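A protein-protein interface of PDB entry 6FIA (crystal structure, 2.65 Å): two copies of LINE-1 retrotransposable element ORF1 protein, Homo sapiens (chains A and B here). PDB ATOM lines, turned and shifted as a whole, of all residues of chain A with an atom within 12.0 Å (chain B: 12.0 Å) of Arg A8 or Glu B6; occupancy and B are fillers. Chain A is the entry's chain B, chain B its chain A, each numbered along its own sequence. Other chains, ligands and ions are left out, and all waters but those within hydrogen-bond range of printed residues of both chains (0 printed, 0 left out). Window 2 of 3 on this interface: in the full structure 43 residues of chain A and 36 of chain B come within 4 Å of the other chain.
Ile A11 touches Lys B14 (O to CG, 3.5 Å). Gly A15 touches Lys B14.
Arg A8 touches Asp B10, but with the chains exchanged Asp A10 does not touch Arg B8 (13.7 Å). Ile A11 touches Lys B14, but with the chains exchanged Lys A14 does not touch Ile B11 (10.1 Å). Gly A15 touches Lys B14, but with the chains exchanged Lys A14 does not touch Gly B15 (8.8 Å). Gly A15 touches Glu B17, but with the chains exchanged Glu A17 does not touch Gly B15 (11.5 Å). Positions printed for both chains: 5, 6, 7, 8, 9, 10, 11, 12, 13, 14, 15, 16 and 17. Of the 6 pairs that touch across the chains among the printed residues, none has its exchanged pair printed and touching as well.
Of the 14 printed residues of chain A, 4 touch a printed residue of chain B. Among the printed residues, 6 pairs touch across the chains. Among the printed residues, Asp or Glu carboxylates within 4 Å of a Lys or Arg side-chain nitrogen of the other chain: Arg A8 with Glu B6 (3.0 Å) and Arg A8 with Asp B10 (3.6 Å).
No residue of chain B comes within 4 Å of Ser A5. Arg A8 touches just these residues of chain B: Glu B6 and Asp B10. No residue of chain B comes within 4 Å of Glu A9. No residue of chain B comes within 4 Å of Asp A10. Printed residues of chain B within 4 Å of Ile A11: Lys B14 (3.5 Å). No residue of chain B comes within 4 Å of Gln A12. Of the printed residues of chain B, Gly A15 touches Lys B14 and Glu B17. Printed residues of chain B within 4 Å of Glu A19: Glu B17 (3.4 Å). No residue of chain A comes within 4 Å of Pro B2. No residue of chain A comes within 4 Å of His B3. No residue of chain A comes within 4 Å of Met B4. Ser B5 touches none of the printed residues of chain A. No residue of chain A comes within 4 Å of Glu B9. Asp B10 touches just one residue of chain A: Arg A8. Of the printed residues of chain A, Lys B14 touches Ile A11 (3.5 Å) and Gly A15 (3.7 Å). Of the printed residues of chain A, Glu B17 touches Gly A15 (3.0 Å) and Glu A19 (3.4 Å). The nearest residue of chain A that does not touch Glu B6 is Gln A12 (7.7 Å). The nearest printed residue of chain A that does not touch Lys B14 is Gln A12 (4.04 Å).
OE1 of Glu B6 lies within salt-bridge range of NH1 of Arg A8, 3.0 Å away. The side-chain carboxylate (OD2) of Asp B10 lies within salt-bridge range of the guanidinium group (NH2) of Arg A8 (3.6 Å). The backbone carbonyl oxygen of Gly A15 sits close to the side-chain carboxylate of Glu B17, at 3.0 Å. The side-chain carboxylate (OE2) of Glu A19 lies close to the side-chain carboxylate (OE1) of Glu B17 (3.4 Å).
OE1 of Glu B6 lies within hydrogen-bond range of ND1 of His B3 (3.4 Å). The backbone NH of Arg A8 is in hydrogen-bond range of the side-chain hydroxyl of Ser A5, at 3.5 Å. O of Arg A8 sits close to NE2 of Gln A12, 3.4 Å away.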
ATOM      1  N   SER A   5      -9.334 -16.291   2.525  1.00  0.00           N
ATOM      2  CA  SER A   5      -9.296 -15.094   3.363  1.00  0.00           C
ATOM      3  C   SER A   5      -7.858 -14.660   3.607  1.00  0.00           C
ATOM      4  O   SER A   5      -7.020 -15.490   3.976  1.00  0.00           O
ATOM      5  CB  SER A   5      -9.995 -15.351   4.701  1.00  0.00           C
ATOM      6  OG  SER A   5      -9.950 -14.233   5.575  1.00  0.00           O
ATOM      7  N   GLU A   6      -7.575 -13.351   3.433  1.00  0.00           N
ATOM      8  CA  GLU A   6      -6.238 -12.791   3.666  1.00  0.00           C
ATOM      9  C   GLU A   6      -5.969 -12.631   5.158  1.00  0.00           C
ATOM     10  O   GLU A   6      -4.853 -12.898   5.609  1.00  0.00           O
ATOM     11  CB  GLU A   6      -6.073 -11.440   2.947  1.00  0.00           C
ATOM     12  CG  GLU A   6      -4.628 -10.968   2.860  1.00  0.00           C
ATOM     13  CD  GLU A   6      -4.437  -9.583   2.274  1.00  0.00           C
ATOM     14  OE1 GLU A   6      -4.730  -9.397   1.069  1.00  0.00           O
ATOM     15  OE2 GLU A   6      -3.969  -8.688   3.014  1.00  0.00           O
ATOM     16  N   LEU A   7      -6.995 -12.189   5.919  1.00  0.00           N
ATOM     17  CA  LEU A   7      -6.898 -11.937   7.361  1.00  0.00           C
ATOM     18  C   LEU A   7      -6.630 -13.200   8.185  1.00  0.00           C
ATOM     19  O   LEU A   7      -5.790 -13.160   9.085  1.00  0.00           O
ATOM     20  CB  LEU A   7      -8.142 -11.193   7.873  1.00  0.00           C
ATOM     21  CG  LEU A   7      -8.052 -10.610   9.279  1.00  0.00           C
ATOM     22  CD1 LEU A   7      -6.972  -9.549   9.369  1.00  0.00           C
ATOM     23  CD2 LEU A   7      -9.362 -10.012   9.688  1.00  0.00           C
ATOM     24  N   ARG A   8      -7.329 -14.325   7.865  1.00  0.00           N
ATOM     25  CA  ARG A   8      -7.158 -15.622   8.549  1.00  0.00           C
ATOM     26  C   ARG A   8      -5.735 -16.184   8.347  1.00  0.00           C
ATOM     27  O   ARG A   8      -5.221 -16.899   9.214  1.00  0.00           O
ATOM     28  CB  ARG A   8      -8.205 -16.637   8.057  1.00  0.00           C
ATOM     29  CG  ARG A   8      -8.351 -17.859   8.966  1.00  0.00           C
ATOM     30  CD  ARG A   8      -8.823 -19.091   8.222  1.00  0.00           C
ATOM     31  NE  ARG A   8     -10.211 -18.976   7.764  1.00  0.00           N
ATOM     32  CZ  ARG A   8     -11.271 -19.341   8.481  1.00  0.00           C
ATOM     33  NH1 ARG A   8     -12.494 -19.216   7.981  1.00  0.00           N
ATOM     34  NH2 ARG A   8     -11.114 -19.832   9.709  1.00  0.00           N
ATOM     35  N   GLU A   9      -5.113 -15.853   7.199  1.00  0.00           N
ATOM     36  CA  GLU A   9      -3.755 -16.263   6.841  1.00  0.00           C
ATOM     37  C   GLU A   9      -2.701 -15.497   7.658  1.00  0.00           C
ATOM     38  O   GLU A   9      -1.759 -16.118   8.149  1.00  0.00           O
ATOM     39  CB  GLU A   9      -3.516 -16.088   5.333  1.00  0.00           C
ATOM     40  CG  GLU A   9      -4.105 -17.217   4.502  1.00  0.00           C
ATOM     41  CD  GLU A   9      -4.123 -16.978   3.003  1.00  0.00           C
ATOM     42  OE1 GLU A   9      -3.038 -16.744   2.423  1.00  0.00           O
ATOM     43  OE2 GLU A   9      -5.215 -17.076   2.398  1.00  0.00           O
ATOM     44  N   ASP A  10      -2.871 -14.153   7.829  1.00  0.00           N
ATOM     45  CA  ASP A  10      -1.947 -13.311   8.615  1.00  0.00           C
ATOM     46  C   ASP A  10      -2.059 -13.629  10.093  1.00  0.00           C
ATOM     47  O   ASP A  10      -1.052 -13.611  10.791  1.00  0.00           O
ATOM     48  CB  ASP A  10      -2.188 -11.807   8.372  1.00  0.00           C
ATOM     49  CG  ASP A  10      -2.257 -11.396   6.902  1.00  0.00           C
ATOM     50  OD1 ASP A  10      -1.590 -12.055   6.061  1.00  0.00           O
ATOM     51  OD2 ASP A  10      -2.962 -10.404   6.593  1.00  0.00           O
ATOM     52  N   ILE A  11      -3.286 -13.958  10.565  1.00  0.00           N
ATOM     53  CA  ILE A  11      -3.551 -14.348  11.958  1.00  0.00           C
ATOM     54  C   ILE A  11      -2.812 -15.651  12.297  1.00  0.00           C
ATOM     55  O   ILE A  11      -2.234 -15.757  13.378  1.00  0.00           O
ATOM     56  CB  ILE A  11      -5.089 -14.380  12.264  1.00  0.00           C
ATOM     57  CG1 ILE A  11      -5.606 -12.936  12.513  1.00  0.00           C
ATOM     58  CG2 ILE A  11      -5.447 -15.346  13.436  1.00  0.00           C
ATOM     59  CD1 ILE A  11      -7.070 -12.756  12.615  1.00  0.00           C
ATOM     60  N   GLN A  12      -2.763 -16.596  11.344  1.00  0.00           N
ATOM     61  CA  GLN A  12      -2.050 -17.860  11.523  1.00  0.00           C
ATOM     62  C   GLN A  12      -0.509 -17.694  11.377  1.00  0.00           C
ATOM     63  O   GLN A  12       0.246 -18.333  12.116  1.00  0.00           O
ATOM     64  CB  GLN A  12      -2.607 -18.937  10.585  1.00  0.00           C
ATOM     65  CG  GLN A  12      -3.961 -19.483  11.045  1.00  0.00           C
ATOM     66  CD  GLN A  12      -4.619 -20.355   9.998  1.00  0.00           C
ATOM     67  OE1 GLN A  12      -3.973 -21.186   9.337  1.00  0.00           O
ATOM     68  NE2 GLN A  12      -5.935 -20.214   9.849  1.00  0.00           N
ATOM     69  N   THR A  13      -0.061 -16.797  10.452  1.00  0.00           N
ATOM     70  CA  THR A  13       1.357 -16.487  10.196  1.00  0.00           C
ATOM     71  C   THR A  13       1.997 -15.754  11.391  1.00  0.00           C
ATOM     72  O   THR A  13       3.110 -16.099  11.790  1.00  0.00           O
ATOM     73  CB  THR A  13       1.504 -15.728   8.862  1.00  0.00           C
ATOM     74  OG1 THR A  13       0.977 -16.545   7.814  1.00  0.00           O
ATOM     75  CG2 THR A  13       2.954 -15.359   8.542  1.00  0.00           C
ATOM     76  N   LYS A  14       1.293 -14.741  11.957  1.00  0.00           N
ATOM     77  CA  LYS A  14       1.768 -14.007  13.142  1.00  0.00           C
ATOM     78  C   LYS A  14       1.725 -14.926  14.383  1.00  0.00           C
ATOM     79  O   LYS A  14       2.515 -14.738  15.310  1.00  0.00           O
ATOM     80  CB  LYS A  14       0.978 -12.692  13.380  1.00  0.00           C
ATOM     81  CG  LYS A  14       0.975 -11.680  12.199  1.00  0.00           C
ATOM     82  CD  LYS A  14       2.291 -10.871  12.011  1.00  0.00           C
ATOM     83  CE  LYS A  14       2.103  -9.570  11.237  1.00  0.00           C
ATOM     84  NZ  LYS A  14       1.593  -9.784   9.847  1.00  0.00           N
ATOM     85  N   GLY A  15       0.845 -15.938  14.343  1.00  0.00           N
ATOM     86  CA  GLY A  15       0.753 -16.989  15.349  1.00  0.00           C
ATOM     87  C   GLY A  15       1.946 -17.928  15.260  1.00  0.00           C
ATOM     88  O   GLY A  15       2.529 -18.286  16.287  1.00  0.00           O
ATOM     89  N   LYS A  16       2.353 -18.280  14.006  1.00  0.00           N
ATOM     90  CA  LYS A  16       3.544 -19.088  13.695  1.00  0.00           C
ATOM     91  C   LYS A  16       4.806 -18.354  14.201  1.00  0.00           C
ATOM     92  O   LYS A  16       5.703 -18.982  14.785  1.00  0.00           O
ATOM     93  CB  LYS A  16       3.683 -19.307  12.167  1.00  0.00           C
ATOM     94  CG  LYS A  16       2.801 -20.396  11.568  1.00  0.00           C
ATOM     95  CD  LYS A  16       2.953 -20.423  10.030  1.00  0.00           C
ATOM     96  CE  LYS A  16       1.808 -21.104   9.317  1.00  0.00           C
ATOM     97  NZ  LYS A  16       1.770 -20.755   7.871  1.00  0.00           N
ATOM     98  N   GLU A  17       4.868 -17.020  13.950  1.00  0.00           N
ATOM     99  CA  GLU A  17       5.973 -16.145  14.351  1.00  0.00           C
ATOM    100  C   GLU A  17       6.213 -16.187  15.859  1.00  0.00           C
ATOM    101  O   GLU A  17       7.358 -16.354  16.277  1.00  0.00           O
ATOM    102  CB  GLU A  17       5.741 -14.694  13.870  1.00  0.00           C
ATOM    103  CG  GLU A  17       6.045 -14.490  12.392  1.00  0.00           C
ATOM    104  CD  GLU A  17       6.657 -13.144  12.057  1.00  0.00           C
ATOM    105  OE1 GLU A  17       5.895 -12.226  11.676  1.00  0.00           O
ATOM    106  OE2 GLU A  17       7.898 -13.006  12.173  1.00  0.00           O
ATOM    107  N   GLU A  19       5.338 -18.612  17.962  1.00  0.00           N
ATOM    108  CA  GLU A  19       5.802 -19.967  18.324  1.00  0.00           C
ATOM    109  C   GLU A  19       7.316 -20.083  18.114  1.00  0.00           C
ATOM    110  O   GLU A  19       8.010 -20.788  18.869  1.00  0.00           O
ATOM    111  CB  GLU A  19       5.098 -21.029  17.474  1.00  0.00           C
ATOM    112  CG  GLU A  19       3.677 -21.343  17.910  1.00  0.00           C
ATOM    113  CD  GLU A  19       2.970 -22.387  17.056  1.00  0.00           C
ATOM    114  OE1 GLU A  19       3.569 -23.464  16.822  1.00  0.00           O
ATOM    115  OE2 GLU A  19       1.806 -22.143  16.648  1.00  0.00           O
ATOM    116  N   PRO B   2     -21.319 -20.393  13.969  1.00  0.00           N
ATOM    117  CA  PRO B   2     -20.326 -21.359  13.479  1.00  0.00           C
ATOM    118  C   PRO B   2     -19.085 -20.688  12.912  1.00  0.00           C
ATOM    119  O   PRO B   2     -17.984 -20.994  13.362  1.00  0.00           O
ATOM    120  CB  PRO B   2     -21.100 -22.172  12.435  1.00  0.00           C
ATOM    121  CG  PRO B   2     -22.496 -22.125  12.905  1.00  0.00           C
ATOM    122  CD  PRO B   2     -22.688 -20.778  13.576  1.00  0.00           C
ATOM    123  N   HIS B   3     -19.252 -19.740  11.965  1.00  0.00           N
ATOM    124  CA  HIS B   3     -18.116 -18.982  11.415  1.00  0.00           C
ATOM    125  C   HIS B   3     -17.615 -17.929  12.406  1.00  0.00           C
ATOM    126  O   HIS B   3     -16.495 -17.434  12.273  1.00  0.00           O
ATOM    127  CB  HIS B   3     -18.440 -18.407  10.037  1.00  0.00           C
ATOM    128  CG  HIS B   3     -18.780 -19.479   9.053  1.00  0.00           C
ATOM    129  ND1 HIS B   3     -18.137 -20.721   9.081  1.00  0.00           N
ATOM    130  CD2 HIS B   3     -19.724 -19.496   8.081  1.00  0.00           C
ATOM    131  CE1 HIS B   3     -18.694 -21.432   8.115  1.00  0.00           C
ATOM    132  NE2 HIS B   3     -19.654 -20.742   7.485  1.00  0.00           N
ATOM    133  N   MET B   4     -18.435 -17.660  13.448  1.00  0.00           N
ATOM    134  CA  MET B   4     -18.086 -16.832  14.585  1.00  0.00           C
ATOM    135  C   MET B   4     -17.226 -17.693  15.499  1.00  0.00           C
ATOM    136  O   MET B   4     -16.184 -17.231  15.964  1.00  0.00           O
ATOM    137  CB  MET B   4     -19.341 -16.383  15.336  1.00  0.00           C
ATOM    138  CG  MET B   4     -19.902 -15.083  14.835  1.00  0.00           C
ATOM    139  SD  MET B   4     -18.947 -13.591  15.256  1.00  0.00           S
ATOM    140  CE  MET B   4     -18.922 -13.713  17.038  1.00  0.00           C
ATOM    141  N   SER B   5     -17.645 -18.978  15.710  1.00  0.00           N
ATOM    142  CA  SER B   5     -16.944 -19.980  16.540  1.00  0.00           C
ATOM    143  C   SER B   5     -15.565 -20.372  15.950  1.00  0.00           C
ATOM    144  O   SER B   5     -14.614 -20.630  16.702  1.00  0.00           O
ATOM    145  CB  SER B   5     -17.815 -21.221  16.726  1.00  0.00           C
ATOM    146  OG  SER B   5     -19.104 -20.871  17.208  1.00  0.00           O
ATOM    147  N   GLU B   6     -15.473 -20.413  14.601  1.00  0.00           N
ATOM    148  CA  GLU B   6     -14.245 -20.679  13.848  1.00  0.00           C
ATOM    149  C   GLU B   6     -13.244 -19.539  14.145  1.00  0.00           C
ATOM    150  O   GLU B   6     -12.095 -19.799  14.478  1.00  0.00           O
ATOM    151  CB  GLU B   6     -14.590 -20.713  12.349  1.00  0.00           C
ATOM    152  CG  GLU B   6     -13.686 -21.544  11.450  1.00  0.00           C
ATOM    153  CD  GLU B   6     -14.222 -21.679  10.028  1.00  0.00           C
ATOM    154  OE1 GLU B   6     -14.711 -20.664   9.474  1.00  0.00           O
ATOM    155  OE2 GLU B   6     -14.190 -22.809   9.482  1.00  0.00           O
ATOM    156  N   LEU B   7     -13.736 -18.285  14.105  1.00  0.00           N
ATOM    157  CA  LEU B   7     -13.011 -17.029  14.344  1.00  0.00           C
ATOM    158  C   LEU B   7     -12.579 -16.854  15.797  1.00  0.00           C
ATOM    159  O   LEU B   7     -11.442 -16.446  16.037  1.00  0.00           O
ATOM    160  CB  LEU B   7     -13.922 -15.845  13.916  1.00  0.00           C
ATOM    161  CG  LEU B   7     -13.471 -14.432  14.270  1.00  0.00           C
ATOM    162  CD1 LEU B   7     -12.142 -14.112  13.644  1.00  0.00           C
ATOM    163  CD2 LEU B   7     -14.485 -13.438  13.833  1.00  0.00           C
ATOM    164  N   ARG B   8     -13.513 -17.078  16.765  1.00  0.00           N
ATOM    165  CA  ARG B   8     -13.248 -16.937  18.214  1.00  0.00           C
ATOM    166  C   ARG B   8     -12.099 -17.858  18.624  1.00  0.00           C
ATOM    167  O   ARG B   8     -11.275 -17.481  19.450  1.00  0.00           O
ATOM    168  CB  ARG B   8     -14.504 -17.286  19.055  1.00  0.00           C
ATOM    169  CG  ARG B   8     -15.697 -16.349  18.861  1.00  0.00           C
ATOM    170  CD  ARG B   8     -16.569 -16.247  20.103  1.00  0.00           C
ATOM    171  NE  ARG B   8     -16.003 -15.313  21.083  1.00  0.00           N
ATOM    172  CZ  ARG B   8     -16.225 -13.997  21.085  1.00  0.00           C
ATOM    173  NH1 ARG B   8     -17.017 -13.448  20.172  1.00  0.00           N
ATOM    174  NH2 ARG B   8     -15.665 -13.226  22.009  1.00  0.00           N
ATOM    175  N   GLU B   9     -12.060 -19.065  18.029  1.00  0.00           N
ATOM    176  CA  GLU B   9     -11.063 -20.065  18.271  1.00  0.00           C
ATOM    177  C   GLU B   9      -9.676 -19.608  17.852  1.00  0.00           C
ATOM    178  O   GLU B   9      -8.736 -19.771  18.637  1.00  0.00           O
ATOM    179  CB  GLU B   9     -11.450 -21.408  17.626  1.00  0.00           C
ATOM    180  CG  GLU B   9     -12.413 -22.208  18.496  1.00  0.00           C
ATOM    181  CD  GLU B   9     -12.692 -23.620  18.028  1.00  0.00           C
ATOM    182  OE1 GLU B   9     -11.866 -24.509  18.330  1.00  0.00           O
ATOM    183  OE2 GLU B   9     -13.753 -23.847  17.399  1.00  0.00           O
ATOM    184  N   ASP B  10      -9.531 -19.016  16.647  1.00  0.00           N
ATOM    185  CA  ASP B  10      -8.217 -18.545  16.174  1.00  0.00           C
ATOM    186  C   ASP B  10      -7.734 -17.342  17.000  1.00  0.00           C
ATOM    187  O   ASP B  10      -6.531 -17.190  17.233  1.00  0.00           O
ATOM    188  CB  ASP B  10      -8.247 -18.201  14.669  1.00  0.00           C
ATOM    189  CG  ASP B  10      -8.856 -19.272  13.776  1.00  0.00           C
ATOM    190  OD1 ASP B  10      -8.735 -20.478  14.117  1.00  0.00           O
ATOM    191  OD2 ASP B  10      -9.440 -18.910  12.725  1.00  0.00           O
ATOM    192  N   ILE B  11      -8.688 -16.486  17.442  1.00  0.00           N
ATOM    193  CA  ILE B  11      -8.409 -15.321  18.279  1.00  0.00           C
ATOM    194  C   ILE B  11      -7.932 -15.784  19.654  1.00  0.00           C
ATOM    195  O   ILE B  11      -6.961 -15.238  20.173  1.00  0.00           O
ATOM    196  CB  ILE B  11      -9.637 -14.349  18.337  1.00  0.00           C
ATOM    197  CG1 ILE B  11      -9.858 -13.599  16.992  1.00  0.00           C
ATOM    198  CG2 ILE B  11      -9.552 -13.354  19.495  1.00  0.00           C
ATOM    199  CD1 ILE B  11      -8.642 -12.891  16.382  1.00  0.00           C
ATOM    200  N   GLN B  12      -8.544 -16.855  20.192  1.00  0.00           N
ATOM    201  CA  GLN B  12      -8.181 -17.386  21.504  1.00  0.00           C
ATOM    202  C   GLN B  12      -6.922 -18.196  21.477  1.00  0.00           C
ATOM    203  O   GLN B  12      -6.129 -18.119  22.421  1.00  0.00           O
ATOM    204  CB  GLN B  12      -9.332 -18.164  22.120  1.00  0.00           C
ATOM    205  CG  GLN B  12     -10.390 -17.246  22.709  1.00  0.00           C
ATOM    206  CD  GLN B  12     -11.631 -17.993  23.084  1.00  0.00           C
ATOM    207  OE1 GLN B  12     -11.598 -18.950  23.874  1.00  0.00           O
ATOM    208  NE2 GLN B  12     -12.762 -17.559  22.538  1.00  0.00           N
ATOM    209  N   THR B  13      -6.711 -18.958  20.390  1.00  0.00           N
ATOM    210  CA  THR B  13      -5.496 -19.738  20.186  1.00  0.00           C
ATOM    211  C   THR B  13      -4.302 -18.794  20.112  1.00  0.00           C
ATOM    212  O   THR B  13      -3.377 -18.920  20.902  1.00  0.00           O
ATOM    213  CB  THR B  13      -5.627 -20.649  18.931  1.00  0.00           C
ATOM    214  OG1 THR B  13      -6.700 -21.564  19.140  1.00  0.00           O
ATOM    215  CG2 THR B  13      -4.333 -21.431  18.607  1.00  0.00           C
ATOM    216  N   LYS B  14      -4.357 -17.808  19.227  1.00  0.00           N
ATOM    217  CA  LYS B  14      -3.239 -16.897  19.060  1.00  0.00           C
ATOM    218  C   LYS B  14      -3.066 -15.959  20.258  1.00  0.00           C
ATOM    219  O   LYS B  14      -1.939 -15.583  20.561  1.00  0.00           O
ATOM    220  CB  LYS B  14      -3.308 -16.157  17.716  1.00  0.00           C
ATOM    221  CG  LYS B  14      -3.307 -17.104  16.467  1.00  0.00           C
ATOM    222  CD  LYS B  14      -2.432 -18.403  16.626  1.00  0.00           C
ATOM    223  CE  LYS B  14      -2.415 -19.297  15.401  1.00  0.00           C
ATOM    224  NZ  LYS B  14      -3.767 -19.825  15.065  1.00  0.00           N
ATOM    225  N   GLY B  15      -4.143 -15.732  21.008  1.00  0.00           N
ATOM    226  CA  GLY B  15      -4.115 -14.940  22.229  1.00  0.00           C
ATOM    227  C   GLY B  15      -3.369 -15.631  23.347  1.00  0.00           C
ATOM    228  O   GLY B  15      -2.523 -15.013  24.003  1.00  0.00           O
ATOM    229  N   LYS B  16      -3.687 -16.932  23.570  1.00  0.00           N
ATOM    230  CA  LYS B  16      -3.032 -17.804  24.559  1.00  0.00           C
ATOM    231  C   LYS B  16      -1.547 -17.952  24.243  1.00  0.00           C
ATOM    232  O   LYS B  16      -0.733 -17.966  25.170  1.00  0.00           O
ATOM    233  CB  LYS B  16      -3.698 -19.209  24.614  1.00  0.00           C
ATOM    234  CG  LYS B  16      -5.003 -19.272  25.424  1.00  0.00           C
ATOM    235  CD  LYS B  16      -5.906 -20.414  24.970  1.00  0.00           C
ATOM    236  CE  LYS B  16      -7.299 -20.339  25.558  1.00  0.00           C
ATOM    237  NZ  LYS B  16      -8.204 -21.371  24.969  1.00  0.00           N
ATOM    238  N   GLU B  17      -1.187 -18.067  22.945  1.00  0.00           N
ATOM    239  CA  GLU B  17       0.218 -18.167  22.540  1.00  0.00           C
ATOM    240  C   GLU B  17       0.970 -16.854  22.879  1.00  0.00           C
ATOM    241  O   GLU B  17       2.105 -16.906  23.353  1.00  0.00           O
ATOM    242  CB  GLU B  17       0.347 -18.466  21.037  1.00  0.00           C
ATOM    243  CG  GLU B  17      -0.113 -19.843  20.588  1.00  0.00           C
ATOM    244  CD  GLU B  17      -0.012 -20.067  19.084  1.00  0.00           C
ATOM    245  OE1 GLU B  17       0.841 -19.408  18.442  1.00  0.00           O
ATOM    246  OE2 GLU B  17      -0.777 -20.904  18.548  1.00  0.00           O
